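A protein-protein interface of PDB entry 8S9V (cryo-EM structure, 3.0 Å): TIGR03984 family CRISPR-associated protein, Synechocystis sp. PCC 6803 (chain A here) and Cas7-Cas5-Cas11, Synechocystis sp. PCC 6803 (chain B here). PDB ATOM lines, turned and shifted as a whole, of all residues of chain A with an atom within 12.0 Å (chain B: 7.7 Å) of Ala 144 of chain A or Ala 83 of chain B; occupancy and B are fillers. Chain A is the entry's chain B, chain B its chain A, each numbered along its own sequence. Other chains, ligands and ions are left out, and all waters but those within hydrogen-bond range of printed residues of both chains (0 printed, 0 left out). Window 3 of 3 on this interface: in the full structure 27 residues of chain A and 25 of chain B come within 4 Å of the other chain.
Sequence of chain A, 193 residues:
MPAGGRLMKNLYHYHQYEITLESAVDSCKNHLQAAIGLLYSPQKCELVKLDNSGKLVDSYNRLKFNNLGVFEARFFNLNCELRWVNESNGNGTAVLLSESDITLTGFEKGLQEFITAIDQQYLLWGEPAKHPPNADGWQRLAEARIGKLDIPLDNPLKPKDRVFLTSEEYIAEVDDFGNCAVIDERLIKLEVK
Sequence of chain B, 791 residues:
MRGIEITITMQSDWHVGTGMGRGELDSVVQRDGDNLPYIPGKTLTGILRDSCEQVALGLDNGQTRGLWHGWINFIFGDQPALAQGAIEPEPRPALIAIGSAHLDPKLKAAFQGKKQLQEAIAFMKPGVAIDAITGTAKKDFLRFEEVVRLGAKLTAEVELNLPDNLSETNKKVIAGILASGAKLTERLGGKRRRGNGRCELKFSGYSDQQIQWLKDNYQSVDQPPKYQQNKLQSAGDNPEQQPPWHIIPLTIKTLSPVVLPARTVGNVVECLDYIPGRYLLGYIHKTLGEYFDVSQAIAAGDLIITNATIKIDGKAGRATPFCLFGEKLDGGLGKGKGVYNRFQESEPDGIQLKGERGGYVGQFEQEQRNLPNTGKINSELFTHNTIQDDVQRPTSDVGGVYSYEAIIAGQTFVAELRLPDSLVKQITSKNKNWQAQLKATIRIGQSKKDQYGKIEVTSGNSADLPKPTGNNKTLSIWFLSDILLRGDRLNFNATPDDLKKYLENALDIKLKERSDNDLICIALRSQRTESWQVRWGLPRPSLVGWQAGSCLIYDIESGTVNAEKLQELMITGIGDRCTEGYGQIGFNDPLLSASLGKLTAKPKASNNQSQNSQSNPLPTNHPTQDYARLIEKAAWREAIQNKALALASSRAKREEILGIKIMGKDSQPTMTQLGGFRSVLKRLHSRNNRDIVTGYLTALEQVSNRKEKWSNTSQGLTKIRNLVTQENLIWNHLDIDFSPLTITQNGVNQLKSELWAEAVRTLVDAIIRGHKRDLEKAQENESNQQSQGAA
OE1 of Glu 88 of chain B is in salt-bridge range of NH2 of Arg 140 of chain A (2.6 Å).
The backbone NH (N) of Lys 148 of chain A sits at hydrogen-bond distance from the backbone carbonyl oxygen (O) of Glu 88 of chain B.
The backbone NH (N) of Ala 129 of chain A is in hydrogen-bond range of the backbone carbonyl oxygen (O) of Arg 140 of chain A (2.8 Å).
O of Glu 127 of chain A lies within hydrogen-bond range of N of Ala 142 of chain A, at 2.7 Å.
Among the printed residues, merely in contact across the chains: Ala 144 of chain A with Ala 83 of chain B, Ile 146 of chain A with Glu 90 of chain B, Gly 147 of chain A with Glu 88 of chain B, Gly 147 of chain A with Ile 87 of chain B, Ala 144 of chain A with Pro 80 of chain B, Gly 147 of chain A with Pro 89 of chain B, Ala 142 of chain A with Ile 87 of chain B and Ala 144 of chain A with Pro 91 of chain B.
Of the printed residues of chain B, Ala 144 of chain A touches Pro 80 (3.7 Å), Ala 83 (3.3 Å) and Pro 91 (3.97 Å).
Of chain A, only Ala 144 comes within 4 Å of Ala 83 of chain B.
Of chain A, only Ala 144 comes within 4 Å of Pro 80 of chain B.
No residue of chain A comes within 4 Å of Ala 81 of chain B.
No residue of chain A comes within 4 Å of Gln 84 of chain B.
No residue of chain A comes within 4 Å of Gly 85 of chain B.
No residue of chain A comes within 4 Å of Ala 86 of chain B.
Pro 91 of chain B touches one residue of chain A.
Of the printed residues of chain B, Ile 146 of chain A touches Glu 90.
Of the printed residues of chain B, Lys 148 of chain A touches Glu 88.
Gln 79 of chain B touches none of the printed residues of chain A.
The nearest residue of chain B that does not touch Ala 144 of chain A is Ile 87 of chain B (4.4 Å).
Of the 17 printed residues of chain A, 6 touch a printed residue of chain B.
Among the printed residues, 10 pairs touch across the chains.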
ATOM      1  N   LEU A 124     -26.051 -36.068 -20.318  1.00  0.00           N
ATOM      2  CA  LEU A 124     -24.882 -35.489 -19.662  1.00  0.00           C
ATOM      3  C   LEU A 124     -25.241 -34.902 -18.301  1.00  0.00           C
ATOM      4  O   LEU A 124     -26.384 -34.562 -18.025  1.00  0.00           O
ATOM      5  CB  LEU A 124     -24.221 -34.419 -20.513  1.00  0.00           C
ATOM      6  CG  LEU A 124     -23.718 -34.801 -21.888  1.00  0.00           C
ATOM      7  CD1 LEU A 124     -22.770 -33.772 -22.377  1.00  0.00           C
ATOM      8  CD2 LEU A 124     -23.068 -36.123 -21.857  1.00  0.00           C
ATOM      9  N   TRP A 125     -24.229 -34.765 -17.454  1.00  0.00           N
ATOM     10  CA  TRP A 125     -24.395 -34.207 -16.117  1.00  0.00           C
ATOM     11  C   TRP A 125     -24.923 -32.781 -16.103  1.00  0.00           C
ATOM     12  O   TRP A 125     -24.338 -31.883 -16.704  1.00  0.00           O
ATOM     13  CB  TRP A 125     -23.060 -34.206 -15.386  1.00  0.00           C
ATOM     14  CG  TRP A 125     -22.493 -35.492 -14.979  1.00  0.00           C
ATOM     15  CD1 TRP A 125     -21.387 -36.082 -15.479  1.00  0.00           C
ATOM     16  CD2 TRP A 125     -22.945 -36.324 -13.921  1.00  0.00           C
ATOM     17  NE1 TRP A 125     -21.135 -37.249 -14.822  1.00  0.00           N
ATOM     18  CE2 TRP A 125     -22.089 -37.419 -13.859  1.00  0.00           C
ATOM     19  CE3 TRP A 125     -24.005 -36.257 -13.030  1.00  0.00           C
ATOM     20  CZ2 TRP A 125     -22.261 -38.431 -12.951  1.00  0.00           C
ATOM     21  CZ3 TRP A 125     -24.172 -37.261 -12.145  1.00  0.00           C
ATOM     22  CH2 TRP A 125     -23.308 -38.332 -12.103  1.00  0.00           C
ATOM     23  N   GLY A 126     -25.998 -32.568 -15.365  1.00  0.00           N
ATOM     24  CA  GLY A 126     -26.408 -31.242 -14.957  1.00  0.00           C
ATOM     25  C   GLY A 126     -27.197 -30.421 -15.959  1.00  0.00           C
ATOM     26  O   GLY A 126     -27.391 -30.775 -17.121  1.00  0.00           O
ATOM     27  N   GLU A 127     -27.665 -29.290 -15.460  1.00  0.00           N
ATOM     28  CA  GLU A 127     -28.435 -28.278 -16.155  1.00  0.00           C
ATOM     29  C   GLU A 127     -27.533 -27.137 -16.572  1.00  0.00           C
ATOM     30  O   GLU A 127     -26.409 -27.014 -16.089  1.00  0.00           O
ATOM     31  CB  GLU A 127     -29.558 -27.781 -15.248  1.00  0.00           C
ATOM     32  CG  GLU A 127     -30.274 -28.911 -14.544  1.00  0.00           C
ATOM     33  CD  GLU A 127     -31.634 -28.529 -14.023  1.00  0.00           C
ATOM     34  OE1 GLU A 127     -32.523 -28.246 -14.842  1.00  0.00           O
ATOM     35  OE2 GLU A 127     -31.839 -28.558 -12.793  1.00  0.00           O
ATOM     36  N   PRO A 128     -27.990 -26.272 -17.467  1.00  0.00           N
ATOM     37  CA  PRO A 128     -27.173 -25.129 -17.872  1.00  0.00           C
ATOM     38  C   PRO A 128     -26.823 -24.203 -16.723  1.00  0.00           C
ATOM     39  O   PRO A 128     -27.646 -23.912 -15.858  1.00  0.00           O
ATOM     40  CB  PRO A 128     -28.049 -24.428 -18.906  1.00  0.00           C
ATOM     41  CG  PRO A 128     -28.880 -25.480 -19.422  1.00  0.00           C
ATOM     42  CD  PRO A 128     -29.210 -26.347 -18.269  1.00  0.00           C
ATOM     43  N   ALA A 129     -25.569 -23.776 -16.702  1.00  0.00           N
ATOM     44  CA  ALA A 129     -25.074 -22.915 -15.652  1.00  0.00           C
ATOM     45  C   ALA A 129     -25.431 -21.475 -15.951  1.00  0.00           C
ATOM     46  O   ALA A 129     -24.554 -20.626 -16.091  1.00  0.00           O
ATOM     47  CB  ALA A 129     -23.605 -23.060 -15.502  1.00  0.00           C
ATOM     48  N   ARG A 140     -21.578 -24.261 -20.423  1.00  0.00           N
ATOM     49  CA  ARG A 140     -21.353 -24.850 -19.116  1.00  0.00           C
ATOM     50  C   ARG A 140     -22.616 -25.492 -18.580  1.00  0.00           C
ATOM     51  O   ARG A 140     -23.638 -24.822 -18.425  1.00  0.00           O
ATOM     52  CB  ARG A 140     -20.827 -23.803 -18.153  1.00  0.00           C
ATOM     53  CG  ARG A 140     -20.427 -24.346 -16.850  1.00  0.00           C
ATOM     54  CD  ARG A 140     -19.673 -23.301 -16.141  1.00  0.00           C
ATOM     55  NE  ARG A 140     -18.379 -23.172 -16.783  1.00  0.00           N
ATOM     56  CZ  ARG A 140     -17.507 -22.216 -16.518  1.00  0.00           C
ATOM     57  NH1 ARG A 140     -16.358 -22.181 -17.162  1.00  0.00           N
ATOM     58  NH2 ARG A 140     -17.802 -21.275 -15.637  1.00  0.00           N
ATOM     59  N   LEU A 141     -22.537 -26.781 -18.301  1.00  0.00           N
ATOM     60  CA  LEU A 141     -23.497 -27.480 -17.471  1.00  0.00           C
ATOM     61  C   LEU A 141     -23.012 -27.421 -16.034  1.00  0.00           C
ATOM     62  O   LEU A 141     -21.825 -27.259 -15.778  1.00  0.00           O
ATOM     63  CB  LEU A 141     -23.630 -28.923 -17.929  1.00  0.00           C
ATOM     64  CG  LEU A 141     -23.969 -29.133 -19.390  1.00  0.00           C
ATOM     65  CD1 LEU A 141     -24.019 -30.574 -19.652  1.00  0.00           C
ATOM     66  CD2 LEU A 141     -25.287 -28.539 -19.680  1.00  0.00           C
ATOM     67  N   ALA A 142     -23.925 -27.578 -15.088  1.00  0.00           N
ATOM     68  CA  ALA A 142     -23.498 -27.656 -13.703  1.00  0.00           C
ATOM     69  C   ALA A 142     -24.448 -28.531 -12.919  1.00  0.00           C
ATOM     70  O   ALA A 142     -25.654 -28.487 -13.136  1.00  0.00           O
ATOM     71  CB  ALA A 142     -23.431 -26.276 -13.069  1.00  0.00           C
ATOM     72  N   GLU A 143     -23.897 -29.278 -11.969  1.00  0.00           N
ATOM     73  CA  GLU A 143     -24.667 -30.007 -10.977  1.00  0.00           C
ATOM     74  C   GLU A 143     -23.951 -30.011  -9.646  1.00  0.00           C
ATOM     75  O   GLU A 143     -22.734 -30.171  -9.600  1.00  0.00           O
ATOM     76  CB  GLU A 143     -24.885 -31.448 -11.377  1.00  0.00           C
ATOM     77  CG  GLU A 143     -25.683 -32.138 -10.343  1.00  0.00           C
ATOM     78  CD  GLU A 143     -26.169 -33.478 -10.762  1.00  0.00           C
ATOM     79  OE1 GLU A 143     -25.992 -33.822 -11.943  1.00  0.00           O
ATOM     80  OE2 GLU A 143     -26.754 -34.175  -9.908  1.00  0.00           O
ATOM     81  N   ALA A 144     -24.694 -29.807  -8.563  1.00  0.00           N
ATOM     82  CA  ALA A 144     -24.045 -29.730  -7.266  1.00  0.00           C
ATOM     83  C   ALA A 144     -23.305 -30.996  -6.893  1.00  0.00           C
ATOM     84  O   ALA A 144     -22.394 -30.945  -6.070  1.00  0.00           O
ATOM     85  CB  ALA A 144     -25.072 -29.450  -6.190  1.00  0.00           C
ATOM     86  N   ARG A 145     -23.675 -32.130  -7.468  1.00  0.00           N
ATOM     87  CA  ARG A 145     -22.928 -33.369  -7.293  1.00  0.00           C
ATOM     88  C   ARG A 145     -21.501 -33.312  -7.806  1.00  0.00           C
ATOM     89  O   ARG A 145     -20.628 -33.985  -7.266  1.00  0.00           O
ATOM     90  CB  ARG A 145     -23.668 -34.474  -8.008  1.00  0.00           C
ATOM     91  CG  ARG A 145     -23.182 -35.788  -7.692  1.00  0.00           C
ATOM     92  CD  ARG A 145     -24.071 -36.786  -8.296  1.00  0.00           C
ATOM     93  NE  ARG A 145     -23.648 -38.102  -7.893  1.00  0.00           N
ATOM     94  CZ  ARG A 145     -24.362 -39.181  -8.115  1.00  0.00           C
ATOM     95  NH1 ARG A 145     -23.947 -40.357  -7.690  1.00  0.00           N
ATOM     96  NH2 ARG A 145     -25.507 -39.065  -8.753  1.00  0.00           N
ATOM     97  N   ILE A 146     -21.237 -32.546  -8.862  1.00  0.00           N
ATOM     98  CA  ILE A 146     -19.951 -32.581  -9.542  1.00  0.00           C
ATOM     99  C   ILE A 146     -19.393 -31.199  -9.826  1.00  0.00           C
ATOM    100  O   ILE A 146     -18.266 -31.085 -10.292  1.00  0.00           O
ATOM    101  CB  ILE A 146     -20.028 -33.412 -10.842  1.00  0.00           C
ATOM    102  CG1 ILE A 146     -20.966 -32.780 -11.851  1.00  0.00           C
ATOM    103  CG2 ILE A 146     -20.492 -34.810 -10.564  1.00  0.00           C
ATOM    104  CD1 ILE A 146     -20.414 -32.752 -13.205  1.00  0.00           C
ATOM    105  N   GLY A 147     -20.133 -30.146  -9.526  1.00  0.00           N
ATOM    106  CA  GLY A 147     -19.804 -28.815  -9.989  1.00  0.00           C
ATOM    107  C   GLY A 147     -20.095 -28.596 -11.457  1.00  0.00           C
ATOM    108  O   GLY A 147     -21.076 -29.104 -11.994  1.00  0.00           O
ATOM    109  N   LYS A 148     -19.265 -27.799 -12.112  1.00  0.00           N
ATOM    110  CA  LYS A 148     -19.439 -27.519 -13.528  1.00  0.00           C
ATOM    111  C   LYS A 148     -18.923 -28.638 -14.421  1.00  0.00           C
ATOM    112  O   LYS A 148     -18.061 -29.427 -14.043  1.00  0.00           O
ATOM    113  CB  LYS A 148     -18.754 -26.212 -13.886  1.00  0.00           C
ATOM    114  CG  LYS A 148     -17.280 -26.280 -13.773  1.00  0.00           C
ATOM    115  CD  LYS A 148     -16.655 -24.993 -14.178  1.00  0.00           C
ATOM    116  CE  LYS A 148     -15.161 -25.088 -14.068  1.00  0.00           C
ATOM    117  NZ  LYS A 148     -14.633 -26.074 -15.053  1.00  0.00           N
ATOM    118  N   LEU A 149     -19.452 -28.664 -15.644  1.00  0.00           N
ATOM    119  CA  LEU A 149     -18.889 -29.400 -16.771  1.00  0.00           C
ATOM    120  C   LEU A 149     -18.971 -28.496 -17.992  1.00  0.00           C
ATOM    121  O   LEU A 149     -20.067 -28.247 -18.486  1.00  0.00           O
ATOM    122  CB  LEU A 149     -19.650 -30.706 -17.002  1.00  0.00           C
ATOM    123  CG  LEU A 149     -19.283 -31.641 -18.159  1.00  0.00           C
ATOM    124  CD1 LEU A 149     -17.931 -32.255 -17.944  1.00  0.00           C
ATOM    125  CD2 LEU A 149     -20.315 -32.717 -18.366  1.00  0.00           C
ATOM    126  N   ARG A 162     -31.372 -29.764 -21.588  1.00  0.00           N
ATOM    127  CA  ARG A 162     -30.463 -30.848 -21.264  1.00  0.00           C
ATOM    128  C   ARG A 162     -29.635 -31.145 -22.496  1.00  0.00           C
ATOM    129  O   ARG A 162     -30.058 -30.884 -23.617  1.00  0.00           O
ATOM    130  CB  ARG A 162     -31.181 -32.130 -20.878  1.00  0.00           C
ATOM    131  CG  ARG A 162     -31.941 -32.151 -19.617  1.00  0.00           C
ATOM    132  CD  ARG A 162     -30.976 -32.060 -18.480  1.00  0.00           C
ATOM    133  NE  ARG A 162     -31.653 -32.197 -17.214  1.00  0.00           N
ATOM    134  CZ  ARG A 162     -32.156 -31.180 -16.553  1.00  0.00           C
ATOM    135  NH1 ARG A 162     -32.749 -31.375 -15.386  1.00  0.00           N
ATOM    136  NH2 ARG A 162     -32.065 -29.968 -17.069  1.00  0.00           N
ATOM    137  N   ASP B  78     -18.990 -29.148   2.398  1.00  0.00           N
ATOM    138  CA  ASP B  78     -20.256 -28.736   1.825  1.00  0.00           C
ATOM    139  C   ASP B  78     -21.283 -29.838   1.868  1.00  0.00           C
ATOM    140  O   ASP B  78     -20.958 -31.020   1.860  1.00  0.00           O
ATOM    141  CB  ASP B  78     -20.090 -28.298   0.383  1.00  0.00           C
ATOM    142  CG  ASP B  78     -19.266 -27.067   0.249  1.00  0.00           C
ATOM    143  OD1 ASP B  78     -19.704 -26.016   0.736  1.00  0.00           O
ATOM    144  OD2 ASP B  78     -18.183 -27.134  -0.352  1.00  0.00           O
ATOM    145  N   GLN B  79     -22.528 -29.437   1.932  1.00  0.00           N
ATOM    146  CA  GLN B  79     -23.614 -30.365   1.739  1.00  0.00           C
ATOM    147  C   GLN B  79     -24.133 -30.138   0.333  1.00  0.00           C
ATOM    148  O   GLN B  79     -25.019 -29.303   0.144  1.00  0.00           O
ATOM    149  CB  GLN B  79     -24.709 -30.097   2.752  1.00  0.00           C
ATOM    150  CG  GLN B  79     -24.232 -30.092   4.159  1.00  0.00           C
ATOM    151  CD  GLN B  79     -25.335 -30.280   5.131  1.00  0.00           C
ATOM    152  OE1 GLN B  79     -25.784 -31.388   5.370  1.00  0.00           O
ATOM    153  NE2 GLN B  79     -25.811 -29.189   5.684  1.00  0.00           N
ATOM    154  N   PRO B  80     -23.600 -30.812  -0.679  1.00  0.00           N
ATOM    155  CA  PRO B  80     -24.363 -31.049  -1.898  1.00  0.00           C
ATOM    156  C   PRO B  80     -25.685 -31.678  -1.549  1.00  0.00           C
ATOM    157  O   PRO B  80     -25.831 -32.195  -0.446  1.00  0.00           O
ATOM    158  CB  PRO B  80     -23.471 -32.006  -2.675  1.00  0.00           C
ATOM    159  CG  PRO B  80     -22.156 -31.719  -2.209  1.00  0.00           C
ATOM    160  CD  PRO B  80     -22.291 -31.460  -0.764  1.00  0.00           C
ATOM    161  N   ALA B  81     -26.649 -31.682  -2.438  1.00  0.00           N
ATOM    162  CA  ALA B  81     -28.001 -32.095  -2.097  1.00  0.00           C
ATOM    163  C   ALA B  81     -28.688 -31.181  -1.114  1.00  0.00           C
ATOM    164  O   ALA B  81     -29.750 -31.525  -0.605  1.00  0.00           O
ATOM    165  CB  ALA B  81     -27.995 -33.509  -1.527  1.00  0.00           C
ATOM    166  N   LEU B  82     -28.104 -30.036  -0.811  1.00  0.00           N
ATOM    167  CA  LEU B  82     -28.847 -28.898  -0.299  1.00  0.00           C
ATOM    168  C   LEU B  82     -28.739 -27.731  -1.259  1.00  0.00           C
ATOM    169  O   LEU B  82     -29.124 -26.614  -0.916  1.00  0.00           O
ATOM    170  CB  LEU B  82     -28.362 -28.487   1.079  1.00  0.00           C
ATOM    171  CG  LEU B  82     -28.451 -29.609   2.085  1.00  0.00           C
ATOM    172  CD1 LEU B  82     -28.079 -29.060   3.425  1.00  0.00           C
ATOM    173  CD2 LEU B  82     -29.792 -30.232   2.081  1.00  0.00           C
ATOM    174  N   ALA B  83     -28.192 -27.965  -2.442  1.00  0.00           N
ATOM    175  CA  ALA B  83     -27.952 -26.899  -3.391  1.00  0.00           C
ATOM    176  C   ALA B  83     -29.249 -26.410  -3.993  1.00  0.00           C
ATOM    177  O   ALA B  83     -30.110 -27.205  -4.374  1.00  0.00           O
ATOM    178  CB  ALA B  83     -27.027 -27.395  -4.492  1.00  0.00           C
ATOM    179  N   GLN B  84     -29.392 -25.089  -4.053  1.00  0.00           N
ATOM    180  CA  GLN B  84     -30.589 -24.434  -4.536  1.00  0.00           C
ATOM    181  C   GLN B  84     -30.396 -23.761  -5.879  1.00  0.00           C
ATOM    182  O   GLN B  84     -31.368 -23.260  -6.447  1.00  0.00           O
ATOM    183  CB  GLN B  84     -31.062 -23.406  -3.510  1.00  0.00           C
ATOM    184  CG  GLN B  84     -31.603 -24.029  -2.254  1.00  0.00           C
ATOM    185  CD  GLN B  84     -31.649 -23.051  -1.115  1.00  0.00           C
ATOM    186  OE1 GLN B  84     -30.756 -22.223  -0.966  1.00  0.00           O
ATOM    187  NE2 GLN B  84     -32.689 -23.134  -0.300  1.00  0.00           N
ATOM    188  N   GLY B  85     -29.181 -23.740  -6.404  1.00  0.00           N
ATOM    189  CA  GLY B  85     -28.924 -23.117  -7.678  1.00  0.00           C
ATOM    190  C   GLY B  85     -27.639 -23.649  -8.256  1.00  0.00           C
ATOM    191  O   GLY B  85     -27.058 -24.601  -7.742  1.00  0.00           O
ATOM    192  N   ALA B  86     -27.211 -23.045  -9.352  1.00  0.00           N
ATOM    193  CA  ALA B  86     -26.024 -23.545 -10.027  1.00  0.00           C
ATOM    194  C   ALA B  86     -24.818 -23.354  -9.132  1.00  0.00           C
ATOM    195  O   ALA B  86     -24.547 -22.241  -8.679  1.00  0.00           O
ATOM    196  CB  ALA B  86     -25.818 -22.832 -11.357  1.00  0.00           C
ATOM    197  N   ILE B  87     -24.105 -24.444  -8.863  1.00  0.00           N
ATOM    198  CA  ILE B  87     -22.843 -24.411  -8.137  1.00  0.00           C
ATOM    199  C   ILE B  87     -21.770 -24.926  -9.069  1.00  0.00           C
ATOM    200  O   ILE B  87     -21.874 -26.046  -9.574  1.00  0.00           O
ATOM    201  CB  ILE B  87     -22.889 -25.234  -6.848  1.00  0.00           C
ATOM    202  CG1 ILE B  87     -23.984 -24.714  -5.930  1.00  0.00           C
ATOM    203  CG2 ILE B  87     -21.574 -25.133  -6.149  1.00  0.00           C
ATOM    204  CD1 ILE B  87     -24.079 -25.450  -4.662  1.00  0.00           C
ATOM    205  N   GLU B  88     -20.768 -24.106  -9.325  1.00  0.00           N
ATOM    206  CA  GLU B  88     -19.703 -24.484 -10.237  1.00  0.00           C
ATOM    207  C   GLU B  88     -18.486 -25.154  -9.612  1.00  0.00           C
ATOM    208  O   GLU B  88     -17.901 -26.032 -10.251  1.00  0.00           O
ATOM    209  CB  GLU B  88     -19.285 -23.275 -11.059  1.00  0.00           C
ATOM    210  CG  GLU B  88     -20.395 -22.859 -11.995  1.00  0.00           C
ATOM    211  CD  GLU B  88     -20.086 -21.617 -12.783  1.00  0.00           C
ATOM    212  OE1 GLU B  88     -18.992 -21.537 -13.375  1.00  0.00           O
ATOM    213  OE2 GLU B  88     -20.959 -20.725 -12.833  1.00  0.00           O
ATOM    214  N   PRO B  89     -18.037 -24.786  -8.418  1.00  0.00           N
ATOM    215  CA  PRO B  89     -16.974 -25.573  -7.793  1.00  0.00           C
ATOM    216  C   PRO B  89     -17.459 -26.926  -7.296  1.00  0.00           C
ATOM    217  O   PRO B  89     -18.580 -27.077  -6.808  1.00  0.00           O
ATOM    218  CB  PRO B  89     -16.521 -24.683  -6.637  1.00  0.00           C
ATOM    219  CG  PRO B  89     -17.680 -23.881  -6.324  1.00  0.00           C
ATOM    220  CD  PRO B  89     -18.377 -23.610  -7.614  1.00  0.00           C
ATOM    221  N   GLU B  90     -16.566 -27.907  -7.375  1.00  0.00           N
ATOM    222  CA  GLU B  90     -16.796 -29.218  -6.792  1.00  0.00           C
ATOM    223  C   GLU B  90     -16.972 -29.111  -5.285  1.00  0.00           C
ATOM    224  O   GLU B  90     -16.409 -28.218  -4.654  1.00  0.00           O
ATOM    225  CB  GLU B  90     -15.645 -30.157  -7.115  1.00  0.00           C
ATOM    226  CG  GLU B  90     -15.506 -30.449  -8.579  1.00  0.00           C
ATOM    227  CD  GLU B  90     -14.806 -29.333  -9.315  1.00  0.00           C
ATOM    228  OE1 GLU B  90     -14.421 -28.348  -8.650  1.00  0.00           O
ATOM    229  OE2 GLU B  90     -14.644 -29.434 -10.554  1.00  0.00           O
ATOM    230  N   PRO B  91     -17.743 -30.003  -4.685  1.00  0.00           N
ATOM    231  CA  PRO B  91     -17.916 -29.952  -3.235  1.00  0.00           C
ATOM    232  C   PRO B  91     -16.617 -30.175  -2.475  1.00  0.00           C
ATOM    233  O   PRO B  91     -15.815 -31.046  -2.813  1.00  0.00           O
ATOM    234  CB  PRO B  91     -18.929 -31.068  -2.976  1.00  0.00           C
ATOM    235  CG  PRO B  91     -18.826 -31.948  -4.132  1.00  0.00           C
ATOM    236  CD  PRO B  91     -18.508 -31.099  -5.284  1.00  0.00           C
